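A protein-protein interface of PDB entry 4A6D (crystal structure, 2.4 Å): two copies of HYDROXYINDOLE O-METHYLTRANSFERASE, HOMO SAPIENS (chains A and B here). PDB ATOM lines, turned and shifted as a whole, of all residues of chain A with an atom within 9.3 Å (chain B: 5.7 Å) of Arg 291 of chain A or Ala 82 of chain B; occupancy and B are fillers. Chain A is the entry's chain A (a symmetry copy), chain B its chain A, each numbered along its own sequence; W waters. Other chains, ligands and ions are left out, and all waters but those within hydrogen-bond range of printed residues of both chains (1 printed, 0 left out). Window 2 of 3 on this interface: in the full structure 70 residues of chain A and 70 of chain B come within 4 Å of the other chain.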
ATOM      1  N   LEU A 285      11.755 -24.910 -36.373  1.00  0.00           N
ATOM      2  CA  LEU A 285      11.488 -25.340 -35.009  1.00  0.00           C
ATOM      3  C   LEU A 285      12.015 -24.393 -33.962  1.00  0.00           C
ATOM      4  O   LEU A 285      13.162 -23.957 -34.034  1.00  0.00           O
ATOM      5  CB  LEU A 285      12.016 -26.778 -34.768  1.00  0.00           C
ATOM      6  CG  LEU A 285      11.331 -27.909 -35.552  1.00  0.00           C
ATOM      7  CD1 LEU A 285      12.056 -29.236 -35.339  1.00  0.00           C
ATOM      8  CD2 LEU A 285       9.872 -28.046 -35.166  1.00  0.00           C
ATOM      9  N   LEU A 286      11.166 -24.073 -32.986  1.00  0.00           N
ATOM     10  CA  LEU A 286      11.556 -23.222 -31.866  1.00  0.00           C
ATOM     11  C   LEU A 286      12.254 -24.082 -30.825  1.00  0.00           C
ATOM     12  O   LEU A 286      11.827 -25.216 -30.606  1.00  0.00           O
ATOM     13  CB  LEU A 286      10.314 -22.582 -31.220  1.00  0.00           C
ATOM     14  CG  LEU A 286       9.988 -21.150 -31.565  1.00  0.00           C
ATOM     15  CD1 LEU A 286       8.833 -20.699 -30.738  1.00  0.00           C
ATOM     16  CD2 LEU A 286      11.160 -20.195 -31.303  1.00  0.00           C
ATOM     17  N   ASP A 287      13.292 -23.552 -30.139  1.00  0.00           N
ATOM     18  CA  ASP A 287      13.939 -24.340 -29.066  1.00  0.00           C
ATOM     19  C   ASP A 287      12.830 -24.605 -28.023  1.00  0.00           C
ATOM     20  O   ASP A 287      11.927 -23.778 -27.888  1.00  0.00           O
ATOM     21  CB  ASP A 287      15.086 -23.537 -28.373  1.00  0.00           C
ATOM     22  CG  ASP A 287      16.353 -23.211 -29.176  1.00  0.00           C
ATOM     23  OD1 ASP A 287      16.565 -23.833 -30.233  1.00  0.00           O
ATOM     24  OD2 ASP A 287      17.144 -22.312 -28.728  1.00  0.00           O
ATOM     25  N   GLU A 288      12.911 -25.696 -27.271  1.00  0.00           N
ATOM     26  CA  GLU A 288      11.923 -26.000 -26.232  1.00  0.00           C
ATOM     27  C   GLU A 288      11.598 -24.891 -25.213  1.00  0.00           C
ATOM     28  O   GLU A 288      10.459 -24.821 -24.750  1.00  0.00           O
ATOM     29  CB  GLU A 288      12.245 -27.315 -25.536  1.00  0.00           C
ATOM     30  CG  GLU A 288      11.898 -28.548 -26.364  1.00  0.00           C
ATOM     31  CD  GLU A 288      10.442 -28.780 -26.700  1.00  0.00           C
ATOM     32  OE1 GLU A 288       9.561 -28.193 -26.030  1.00  0.00           O
ATOM     33  OE2 GLU A 288      10.184 -29.571 -27.634  1.00  0.00           O
ATOM     34  N   ASP A 289      12.579 -24.036 -24.863  1.00  0.00           N
ATOM     35  CA  ASP A 289      12.372 -22.910 -23.940  1.00  0.00           C
ATOM     36  C   ASP A 289      11.731 -21.684 -24.631  1.00  0.00           C
ATOM     37  O   ASP A 289      11.460 -20.680 -23.964  1.00  0.00           O
ATOM     38  CB  ASP A 289      13.663 -22.534 -23.165  1.00  0.00           C
ATOM     39  CG  ASP A 289      14.917 -22.117 -23.939  1.00  0.00           C
ATOM     40  OD1 ASP A 289      14.793 -21.710 -25.112  1.00  0.00           O
ATOM     41  OD2 ASP A 289      16.013 -22.123 -23.337  1.00  0.00           O
ATOM     42  N   ARG A 290      11.468 -21.795 -25.966  1.00  0.00           N
ATOM     43  CA  ARG A 290      10.908 -20.756 -26.840  1.00  0.00           C
ATOM     44  C   ARG A 290      11.827 -19.529 -26.941  1.00  0.00           C
ATOM     45  O   ARG A 290      11.464 -18.521 -27.545  1.00  0.00           O
ATOM     46  CB  ARG A 290       9.439 -20.392 -26.484  1.00  0.00           C
ATOM     47  CG  ARG A 290       8.501 -21.605 -26.456  1.00  0.00           C
ATOM     48  CD  ARG A 290       7.034 -21.227 -26.437  1.00  0.00           C
ATOM     49  NE  ARG A 290       6.641 -20.604 -25.175  1.00  0.00           N
ATOM     50  CZ  ARG A 290       6.213 -21.269 -24.108  1.00  0.00           C
ATOM     51  NH1 ARG A 290       6.118 -22.596 -24.138  1.00  0.00           N
ATOM     52  NH2 ARG A 290       5.883 -20.617 -23.002  1.00  0.00           N
ATOM     53  N   ARG A 291      13.050 -19.658 -26.413  1.00  0.00           N
ATOM     54  CA  ARG A 291      14.027 -18.583 -26.398  1.00  0.00           C
ATOM     55  C   ARG A 291      15.104 -18.619 -27.493  1.00  0.00           C
ATOM     56  O   ARG A 291      16.141 -18.003 -27.366  1.00  0.00           O
ATOM     57  CB  ARG A 291      14.597 -18.382 -24.992  1.00  0.00           C
ATOM     58  CG  ARG A 291      14.566 -16.893 -24.600  1.00  0.00           C
ATOM     59  CD  ARG A 291      14.628 -16.679 -23.102  1.00  0.00           C
ATOM     60  NE  ARG A 291      13.428 -17.183 -22.423  1.00  0.00           N
ATOM     61  CZ  ARG A 291      13.362 -18.330 -21.753  1.00  0.00           C
ATOM     62  NH1 ARG A 291      14.424 -19.121 -21.670  1.00  0.00           N
ATOM     63  NH2 ARG A 291      12.239 -18.686 -21.153  1.00  0.00           N
ATOM     64  N   GLY A 292      14.811 -19.282 -28.591  1.00  0.00           N
ATOM     65  CA  GLY A 292      15.715 -19.329 -29.725  1.00  0.00           C
ATOM     66  C   GLY A 292      15.270 -20.373 -30.721  1.00  0.00           C
ATOM     67  O   GLY A 292      14.411 -21.198 -30.411  1.00  0.00           O
ATOM     68  N   PRO A 293      15.869 -20.421 -31.918  1.00  0.00           N
ATOM     69  CA  PRO A 293      16.892 -19.486 -32.438  1.00  0.00           C
ATOM     70  C   PRO A 293      16.256 -18.112 -32.655  1.00  0.00           C
ATOM     71  O   PRO A 293      15.031 -18.015 -32.838  1.00  0.00           O
ATOM     72  CB  PRO A 293      17.312 -20.129 -33.771  1.00  0.00           C
ATOM     73  CG  PRO A 293      16.730 -21.601 -33.737  1.00  0.00           C
ATOM     74  CD  PRO A 293      15.515 -21.486 -32.887  1.00  0.00           C
ATOM     75  N   LEU A 294      17.078 -17.037 -32.620  1.00  0.00           N
ATOM     76  CA  LEU A 294      16.602 -15.679 -32.787  1.00  0.00           C
ATOM     77  C   LEU A 294      15.763 -15.493 -34.060  1.00  0.00           C
ATOM     78  O   LEU A 294      14.675 -14.905 -33.999  1.00  0.00           O
ATOM     79  CB  LEU A 294      17.785 -14.699 -32.720  1.00  0.00           C
ATOM     80  CG  LEU A 294      17.532 -13.208 -33.057  1.00  0.00           C
ATOM     81  CD1 LEU A 294      16.374 -12.622 -32.253  1.00  0.00           C
ATOM     82  CD2 LEU A 294      18.802 -12.420 -32.830  1.00  0.00           C
ATOM     83  N   LEU A 295      16.257 -16.005 -35.197  1.00  0.00           N
ATOM     84  CA  LEU A 295      15.565 -15.878 -36.475  1.00  0.00           C
ATOM     85  C   LEU A 295      14.153 -16.515 -36.386  1.00  0.00           C
ATOM     86  O   LEU A 295      13.215 -15.939 -36.903  1.00  0.00           O
ATOM     87  CB  LEU A 295      16.435 -16.495 -37.603  1.00  0.00           C
ATOM     88  CG  LEU A 295      15.876 -16.385 -39.041  1.00  0.00           C
ATOM     89  CD1 LEU A 295      16.991 -16.340 -40.052  1.00  0.00           C
ATOM     90  CD2 LEU A 295      15.014 -17.580 -39.372  1.00  0.00           C
ATOM     91  N   THR A 296      14.011 -17.667 -35.689  1.00  0.00           N
ATOM     92  CA  THR A 296      12.735 -18.377 -35.488  1.00  0.00           C
ATOM     93  C   THR A 296      11.796 -17.574 -34.603  1.00  0.00           C
ATOM     94  O   THR A 296      10.602 -17.507 -34.888  1.00  0.00           O
ATOM     95  CB  THR A 296      12.973 -19.796 -34.962  1.00  0.00           C
ATOM     96  OG1 THR A 296      13.860 -20.462 -35.859  1.00  0.00           O
ATOM     97  CG2 THR A 296      11.695 -20.593 -34.854  1.00  0.00           C
ATOM     98  N   GLN A 297      12.335 -16.979 -33.523  1.00  0.00           N
ATOM     99  CA  GLN A 297      11.572 -16.103 -32.630  1.00  0.00           C
ATOM    100  C   GLN A 297      11.042 -14.891 -33.441  1.00  0.00           C
ATOM    101  O   GLN A 297       9.873 -14.513 -33.277  1.00  0.00           O
ATOM    102  CB  GLN A 297      12.458 -15.587 -31.490  1.00  0.00           C
ATOM    103  CG  GLN A 297      12.829 -16.613 -30.434  1.00  0.00           C
ATOM    104  CD  GLN A 297      13.839 -15.968 -29.518  1.00  0.00           C
ATOM    105  OE1 GLN A 297      15.014 -15.824 -29.846  1.00  0.00           O
ATOM    106  NE2 GLN A 297      13.396 -15.467 -28.396  1.00  0.00           N
ATOM    107  N   LEU A 298      11.886 -14.319 -34.342  1.00  0.00           N
ATOM    108  CA  LEU A 298      11.462 -13.177 -35.163  1.00  0.00           C
ATOM    109  C   LEU A 298      10.336 -13.610 -36.091  1.00  0.00           C
ATOM    110  O   LEU A 298       9.323 -12.920 -36.186  1.00  0.00           O
ATOM    111  CB  LEU A 298      12.633 -12.513 -35.936  1.00  0.00           C
ATOM    112  CG  LEU A 298      13.728 -11.792 -35.118  1.00  0.00           C
ATOM    113  CD1 LEU A 298      14.905 -11.486 -35.979  1.00  0.00           C
ATOM    114  CD2 LEU A 298      13.221 -10.494 -34.498  1.00  0.00           C
ATOM    115  N   THR A 313       7.448 -25.302 -30.909  1.00  0.00           N
ATOM    116  CA  THR A 313       8.478 -26.231 -30.424  1.00  0.00           C
ATOM    117  C   THR A 313       8.162 -27.652 -30.885  1.00  0.00           C
ATOM    118  O   THR A 313       6.980 -27.978 -31.126  1.00  0.00           O
ATOM    119  CB  THR A 313       8.576 -26.215 -28.869  1.00  0.00           C
ATOM    120  OG1 THR A 313       7.405 -26.800 -28.297  1.00  0.00           O
ATOM    121  CG2 THR A 313       8.872 -24.799 -28.279  1.00  0.00           C
ATOM    122  N   LYS A 333      16.602 -31.717 -36.771  1.00  0.00           N
ATOM    123  CA  LYS A 333      17.095 -30.337 -36.851  1.00  0.00           C
ATOM    124  C   LYS A 333      18.190 -30.356 -37.918  1.00  0.00           C
ATOM    125  O   LYS A 333      19.203 -31.043 -37.747  1.00  0.00           O
ATOM    126  CB  LYS A 333      17.586 -29.780 -35.485  1.00  0.00           C
ATOM    127  CG  LYS A 333      16.473 -29.004 -34.750  1.00  0.00           C
ATOM    128  CD  LYS A 333      16.991 -27.770 -33.984  1.00  0.00           C
ATOM    129  CE  LYS A 333      15.890 -26.763 -33.674  1.00  0.00           C
ATOM    130  NZ  LYS A 333      16.390 -25.375 -33.400  1.00  0.00           N
ATOM    131  N   LEU B  44      10.348  -9.427 -13.171  1.00  0.00           N
ATOM    132  CA  LEU B  44       8.936  -9.713 -13.474  1.00  0.00           C
ATOM    133  C   LEU B  44       8.714 -10.847 -14.481  1.00  0.00           C
ATOM    134  O   LEU B  44       9.473 -10.956 -15.449  1.00  0.00           O
ATOM    135  CB  LEU B  44       8.243  -8.455 -14.044  1.00  0.00           C
ATOM    136  CG  LEU B  44       8.197  -7.171 -13.237  1.00  0.00           C
ATOM    137  CD1 LEU B  44       7.622  -6.060 -14.080  1.00  0.00           C
ATOM    138  CD2 LEU B  44       7.371  -7.341 -11.974  1.00  0.00           C
ATOM    139  N   ASP B  45       7.612 -11.615 -14.311  1.00  0.00           N
ATOM    140  CA  ASP B  45       7.225 -12.668 -15.265  1.00  0.00           C
ATOM    141  C   ASP B  45       6.399 -12.061 -16.421  1.00  0.00           C
ATOM    142  O   ASP B  45       6.056 -10.875 -16.354  1.00  0.00           O
ATOM    143  CB  ASP B  45       6.482 -13.841 -14.578  1.00  0.00           C
ATOM    144  CG  ASP B  45       5.215 -13.504 -13.801  1.00  0.00           C
ATOM    145  OD1 ASP B  45       4.463 -12.599 -14.237  1.00  0.00           O
ATOM    146  OD2 ASP B  45       4.935 -14.195 -12.801  1.00  0.00           O
ATOM    147  N   VAL B  46       6.089 -12.867 -17.469  1.00  0.00           N
ATOM    148  CA  VAL B  46       5.313 -12.482 -18.671  1.00  0.00           C
ATOM    149  C   VAL B  46       3.972 -11.816 -18.300  1.00  0.00           C
ATOM    150  O   VAL B  46       3.693 -10.712 -18.763  1.00  0.00           O
ATOM    151  CB  VAL B  46       5.127 -13.669 -19.681  1.00  0.00           C
ATOM    152  CG1 VAL B  46       4.235 -13.281 -20.865  1.00  0.00           C
ATOM    153  CG2 VAL B  46       6.471 -14.191 -20.181  1.00  0.00           C
ATOM    154  N   ASP B  65      11.214 -12.453 -24.952  1.00  0.00           N
ATOM    155  CA  ASP B  65      12.130 -13.512 -25.375  1.00  0.00           C
ATOM    156  C   ASP B  65      13.082 -13.050 -26.459  1.00  0.00           C
ATOM    157  O   ASP B  65      14.276 -13.349 -26.373  1.00  0.00           O
ATOM    158  CB  ASP B  65      11.391 -14.799 -25.750  1.00  0.00           C
ATOM    159  CG  ASP B  65      10.790 -15.548 -24.568  1.00  0.00           C
ATOM    160  OD1 ASP B  65      11.227 -15.294 -23.415  1.00  0.00           O
ATOM    161  OD2 ASP B  65       9.903 -16.415 -24.800  1.00  0.00           O
ATOM    162  N   VAL B  68      15.722 -10.846 -24.768  1.00  0.00           N
ATOM    163  CA  VAL B  68      16.702 -11.679 -24.067  1.00  0.00           C
ATOM    164  C   VAL B  68      17.776 -12.165 -25.065  1.00  0.00           C
ATOM    165  O   VAL B  68      18.962 -11.961 -24.805  1.00  0.00           O
ATOM    166  CB  VAL B  68      16.055 -12.845 -23.285  1.00  0.00           C
ATOM    167  CG1 VAL B  68      17.118 -13.701 -22.610  1.00  0.00           C
ATOM    168  CG2 VAL B  68      15.054 -12.330 -22.258  1.00  0.00           C
ATOM    169  N   SER B  69      17.359 -12.737 -26.224  1.00  0.00           N
ATOM    170  CA  SER B  69      18.252 -13.184 -27.306  1.00  0.00           C
ATOM    171  C   SER B  69      19.116 -12.033 -27.856  1.00  0.00           C
ATOM    172  O   SER B  69      20.279 -12.256 -28.213  1.00  0.00           O
ATOM    173  CB  SER B  69      17.443 -13.807 -28.440  1.00  0.00           C
ATOM    174  OG  SER B  69      16.813 -15.000 -28.009  1.00  0.00           O
ATOM    175  N   VAL B  75      17.256 -13.162 -18.439  1.00  0.00           N
ATOM    176  CA  VAL B  75      16.189 -14.005 -17.913  1.00  0.00           C
ATOM    177  C   VAL B  75      16.769 -14.904 -16.831  1.00  0.00           C
ATOM    178  O   VAL B  75      17.982 -15.125 -16.800  1.00  0.00           O
ATOM    179  CB  VAL B  75      15.391 -14.760 -19.023  1.00  0.00           C
ATOM    180  CG1 VAL B  75      16.205 -15.884 -19.655  1.00  0.00           C
ATOM    181  CG2 VAL B  75      14.058 -15.282 -18.502  1.00  0.00           C
ATOM    182  N   GLU B  76      15.915 -15.350 -15.905  1.00  0.00           N
ATOM    183  CA  GLU B  76      16.256 -16.267 -14.822  1.00  0.00           C
ATOM    184  C   GLU B  76      15.053 -17.153 -14.566  1.00  0.00           C
ATOM    185  O   GLU B  76      13.926 -16.792 -14.919  1.00  0.00           O
ATOM    186  CB  GLU B  76      16.767 -15.535 -13.550  1.00  0.00           C
ATOM    187  CG  GLU B  76      15.726 -15.170 -12.497  1.00  0.00           C
ATOM    188  CD  GLU B  76      16.196 -14.172 -11.452  1.00  0.00           C
ATOM    189  OE1 GLU B  76      16.763 -14.603 -10.422  1.00  0.00           O
ATOM    190  OE2 GLU B  76      15.991 -12.953 -11.664  1.00  0.00           O
ATOM    191  N   THR B  77      15.285 -18.317 -13.984  1.00  0.00           N
ATOM    192  CA  THR B  77      14.205 -19.241 -13.717  1.00  0.00           C
ATOM    193  C   THR B  77      13.954 -19.358 -12.216  1.00  0.00           C
ATOM    194  O   THR B  77      14.906 -19.459 -11.437  1.00  0.00           O
ATOM    195  CB  THR B  77      14.500 -20.560 -14.430  1.00  0.00           C
ATOM    196  OG1 THR B  77      14.858 -20.260 -15.786  1.00  0.00           O
ATOM    197  CG2 THR B  77      13.320 -21.541 -14.383  1.00  0.00           C
ATOM    198  N   ARG B  78      12.668 -19.289 -11.819  1.00  0.00           N
ATOM    199  CA  ARG B  78      12.191 -19.468 -10.442  1.00  0.00           C
ATOM    200  C   ARG B  78      10.904 -20.282 -10.536  1.00  0.00           C
ATOM    201  O   ARG B  78       9.926 -19.815 -11.140  1.00  0.00           O
ATOM    202  CB  ARG B  78      11.952 -18.137  -9.716  1.00  0.00           C
ATOM    203  CG  ARG B  78      13.207 -17.369  -9.329  1.00  0.00           C
ATOM    204  CD  ARG B  78      12.812 -15.988  -8.841  1.00  0.00           C
ATOM    205  NE  ARG B  78      13.949 -15.075  -8.711  1.00  0.00           N
ATOM    206  CZ  ARG B  78      13.836 -13.784  -8.419  1.00  0.00           C
ATOM    207  NH1 ARG B  78      12.640 -13.240  -8.233  1.00  0.00           N
ATOM    208  NH2 ARG B  78      14.920 -13.024  -8.315  1.00  0.00           N
ATOM    209  N   GLY B  80       8.165 -22.718 -11.777  1.00  0.00           N
ATOM    210  CA  GLY B  80       7.659 -22.927 -13.132  1.00  0.00           C
ATOM    211  C   GLY B  80       7.437 -21.639 -13.911  1.00  0.00           C
ATOM    212  O   GLY B  80       6.412 -21.501 -14.592  1.00  0.00           O
ATOM    213  N   LYS B  81       8.400 -20.678 -13.822  1.00  0.00           N
ATOM    214  CA  LYS B  81       8.294 -19.373 -14.475  1.00  0.00           C
ATOM    215  C   LYS B  81       9.625 -18.657 -14.737  1.00  0.00           C
ATOM    216  O   LYS B  81      10.517 -18.627 -13.877  1.00  0.00           O
ATOM    217  CB  LYS B  81       7.400 -18.436 -13.636  1.00  0.00           C
ATOM    218  CG  LYS B  81       5.995 -18.234 -14.186  1.00  0.00           C
ATOM    219  CD  LYS B  81       5.079 -17.593 -13.139  1.00  0.00           C
ATOM    220  CE  LYS B  81       3.611 -17.866 -13.395  1.00  0.00           C
ATOM    221  NZ  LYS B  81       3.244 -19.300 -13.192  1.00  0.00           N
ATOM    222  N   ALA B  82       9.702 -18.002 -15.915  1.00  0.00           N
ATOM    223  CA  ALA B  82      10.802 -17.130 -16.349  1.00  0.00           C
ATOM    224  C   ALA B  82      10.549 -15.767 -15.748  1.00  0.00           C
ATOM    225  O   ALA B  82       9.401 -15.319 -15.709  1.00  0.00           O
ATOM    226  CB  ALA B  82      10.820 -17.006 -17.868  1.00  0.00           C
ATOM    227  N   PHE B  83      11.625 -15.124 -15.269  1.00  0.00           N
ATOM    228  CA  PHE B  83      11.632 -13.783 -14.688  1.00  0.00           C
ATOM    229  C   PHE B  83      12.659 -12.923 -15.403  1.00  0.00           C
ATOM    230  O   PHE B  83      13.833 -13.286 -15.499  1.00  0.00           O
ATOM    231  CB  PHE B  83      11.865 -13.825 -13.171  1.00  0.00           C
ATOM    232  CG  PHE B  83      10.669 -14.357 -12.421  1.00  0.00           C
ATOM    233  CD1 PHE B  83       9.636 -13.512 -12.039  1.00  0.00           C
ATOM    234  CD2 PHE B  83      10.562 -15.709 -12.120  1.00  0.00           C
ATOM    235  CE1 PHE B  83       8.519 -14.008 -11.364  1.00  0.00           C
ATOM    236  CE2 PHE B  83       9.443 -16.205 -11.445  1.00  0.00           C
ATOM    237  CZ  PHE B  83       8.437 -15.345 -11.058  1.00  0.00           C
ATOM    238  N   TYR B  84      12.195 -11.795 -15.938  1.00  0.00           N
ATOM    239  CA  TYR B  84      12.992 -10.872 -16.735  1.00  0.00           C
ATOM    240  C   TYR B  84      13.481  -9.712 -15.932  1.00  0.00           C
ATOM    241  O   TYR B  84      12.786  -9.244 -15.034  1.00  0.00           O
ATOM    242  CB  TYR B  84      12.179 -10.386 -17.939  1.00  0.00           C
ATOM    243  CG  TYR B  84      11.655 -11.526 -18.784  1.00  0.00           C
ATOM    244  CD1 TYR B  84      10.434 -12.135 -18.495  1.00  0.00           C
ATOM    245  CD2 TYR B  84      12.413 -12.049 -19.828  1.00  0.00           C
ATOM    246  CE1 TYR B  84       9.983 -13.242 -19.218  1.00  0.00           C
ATOM    247  CE2 TYR B  84      11.965 -13.146 -20.568  1.00  0.00           C
ATOM    248  CZ  TYR B  84      10.752 -13.739 -20.255  1.00  0.00           C
ATOM    249  OH  TYR B  84      10.292 -14.763 -21.029  1.00  0.00           O
HETATM  250  O   HOH W   1       9.133 -17.040 -27.542  1.00  0.00           O
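Of the 15 printed residues of chain B, 5 touch a printed residue of chain A. Hydrophobic or aromatic side chains of chain B that line the printed part of chain A: Val 68, Val 75 and Ala 82. Along chain B the printed residues that touch a printed residue of chain A span positions 65 to 82. Among the printed residues, Asp or Glu carboxylates within 4 Å of a Lys or Arg side-chain nitrogen of the other chain: Arg 291 of chain A with Asp 65 of chain B (3.1 Å).
Water W1 lies within hydrogen-bond range of the backbone carbonyl oxygen of Arg 290 of chain A and the side-chain carboxylate of Asp 65 of chain B.
Arg 290 of chain A touches Asp 65 of chain B. Val 68 of chain B touches Arg 291 of chain A. Arg 291 of chain A touches Val 75 of chain B. Arg 291 of chain A touches Ala 82 of chain B.
No position is printed for both chains. Of the 8 pairs that touch across the chains among the printed residues, none has its exchanged pair printed and touching as well.
Printed residues of chain B within 4 Å of Arg 290 of chain A: Asp 65 (3.8 Å). Arg 291 of chain A touches just these residues of chain B: Asp 65 (3.1 Å), Val 68 (3.9 Å), Ser 69 (3.1 Å), Val 75 (3.9 Å) and Ala 82 (3.95 Å). Of the printed residues of chain A, Asp 65 of chain B touches Arg 290 (3.8 Å), Arg 291 (3.1 Å) and Gln 297 (3.1 Å). Of the printed residues of chain A, Val 68 of chain B touches Arg 291 (3.9 Å). Of the printed residues of chain A, Ser 69 of chain B touches Arg 291 and Gln 297. Of chain A, only Arg 291 comes within 4 Å of Ala 82 of chain B. No residue of chain A comes within 4 Å of Phe 83 of chain B. The nearest residue of chain B that does not touch Arg 291 of chain A is Tyr 84 of chain B (4.2 Å). The nearest printed residue of chain A that does not touch Val 75 of chain B is Asp 289 of chain A (7.2 Å).
The side-chain hydroxyl of Ser 69 of chain B lies within hydrogen-bond range of the side-chain amide oxygen of Gln 297 of chain A (2.7 Å). The side-chain hydroxyl of Ser 69 of chain B is in hydrogen-bond range of the backbone carbonyl oxygen of Arg 291 of chain A (3.1 Å). The side-chain amide nitrogen of Gln 297 of chain A lies within hydrogen-bond range of the backbone carbonyl oxygen of Asp 65 of chain B, 3.1 Å away. The side-chain carboxylate (OD1) of Asp 65 of chain B lies within salt-bridge range of the guanidinium group (NE) of Arg 291 of chain A, 3.1 Å away.
O of Arg 291 of chain A sits close to OE1 of Gln 297 of chain A (3.5 Å). OD1 of Asp 65 of chain B sits at hydrogen-bond distance from OH of Tyr 84 of chain B (2.6 Å). The side-chain carboxylate (OD2) of Asp 289 of chain A is in salt-bridge range of the guanidinium group (NH1) of Arg 291 of chain A, at 3.8 Å. O of Asp 65 of chain B lies within hydrogen-bond range of OG of Ser 69 of chain B.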
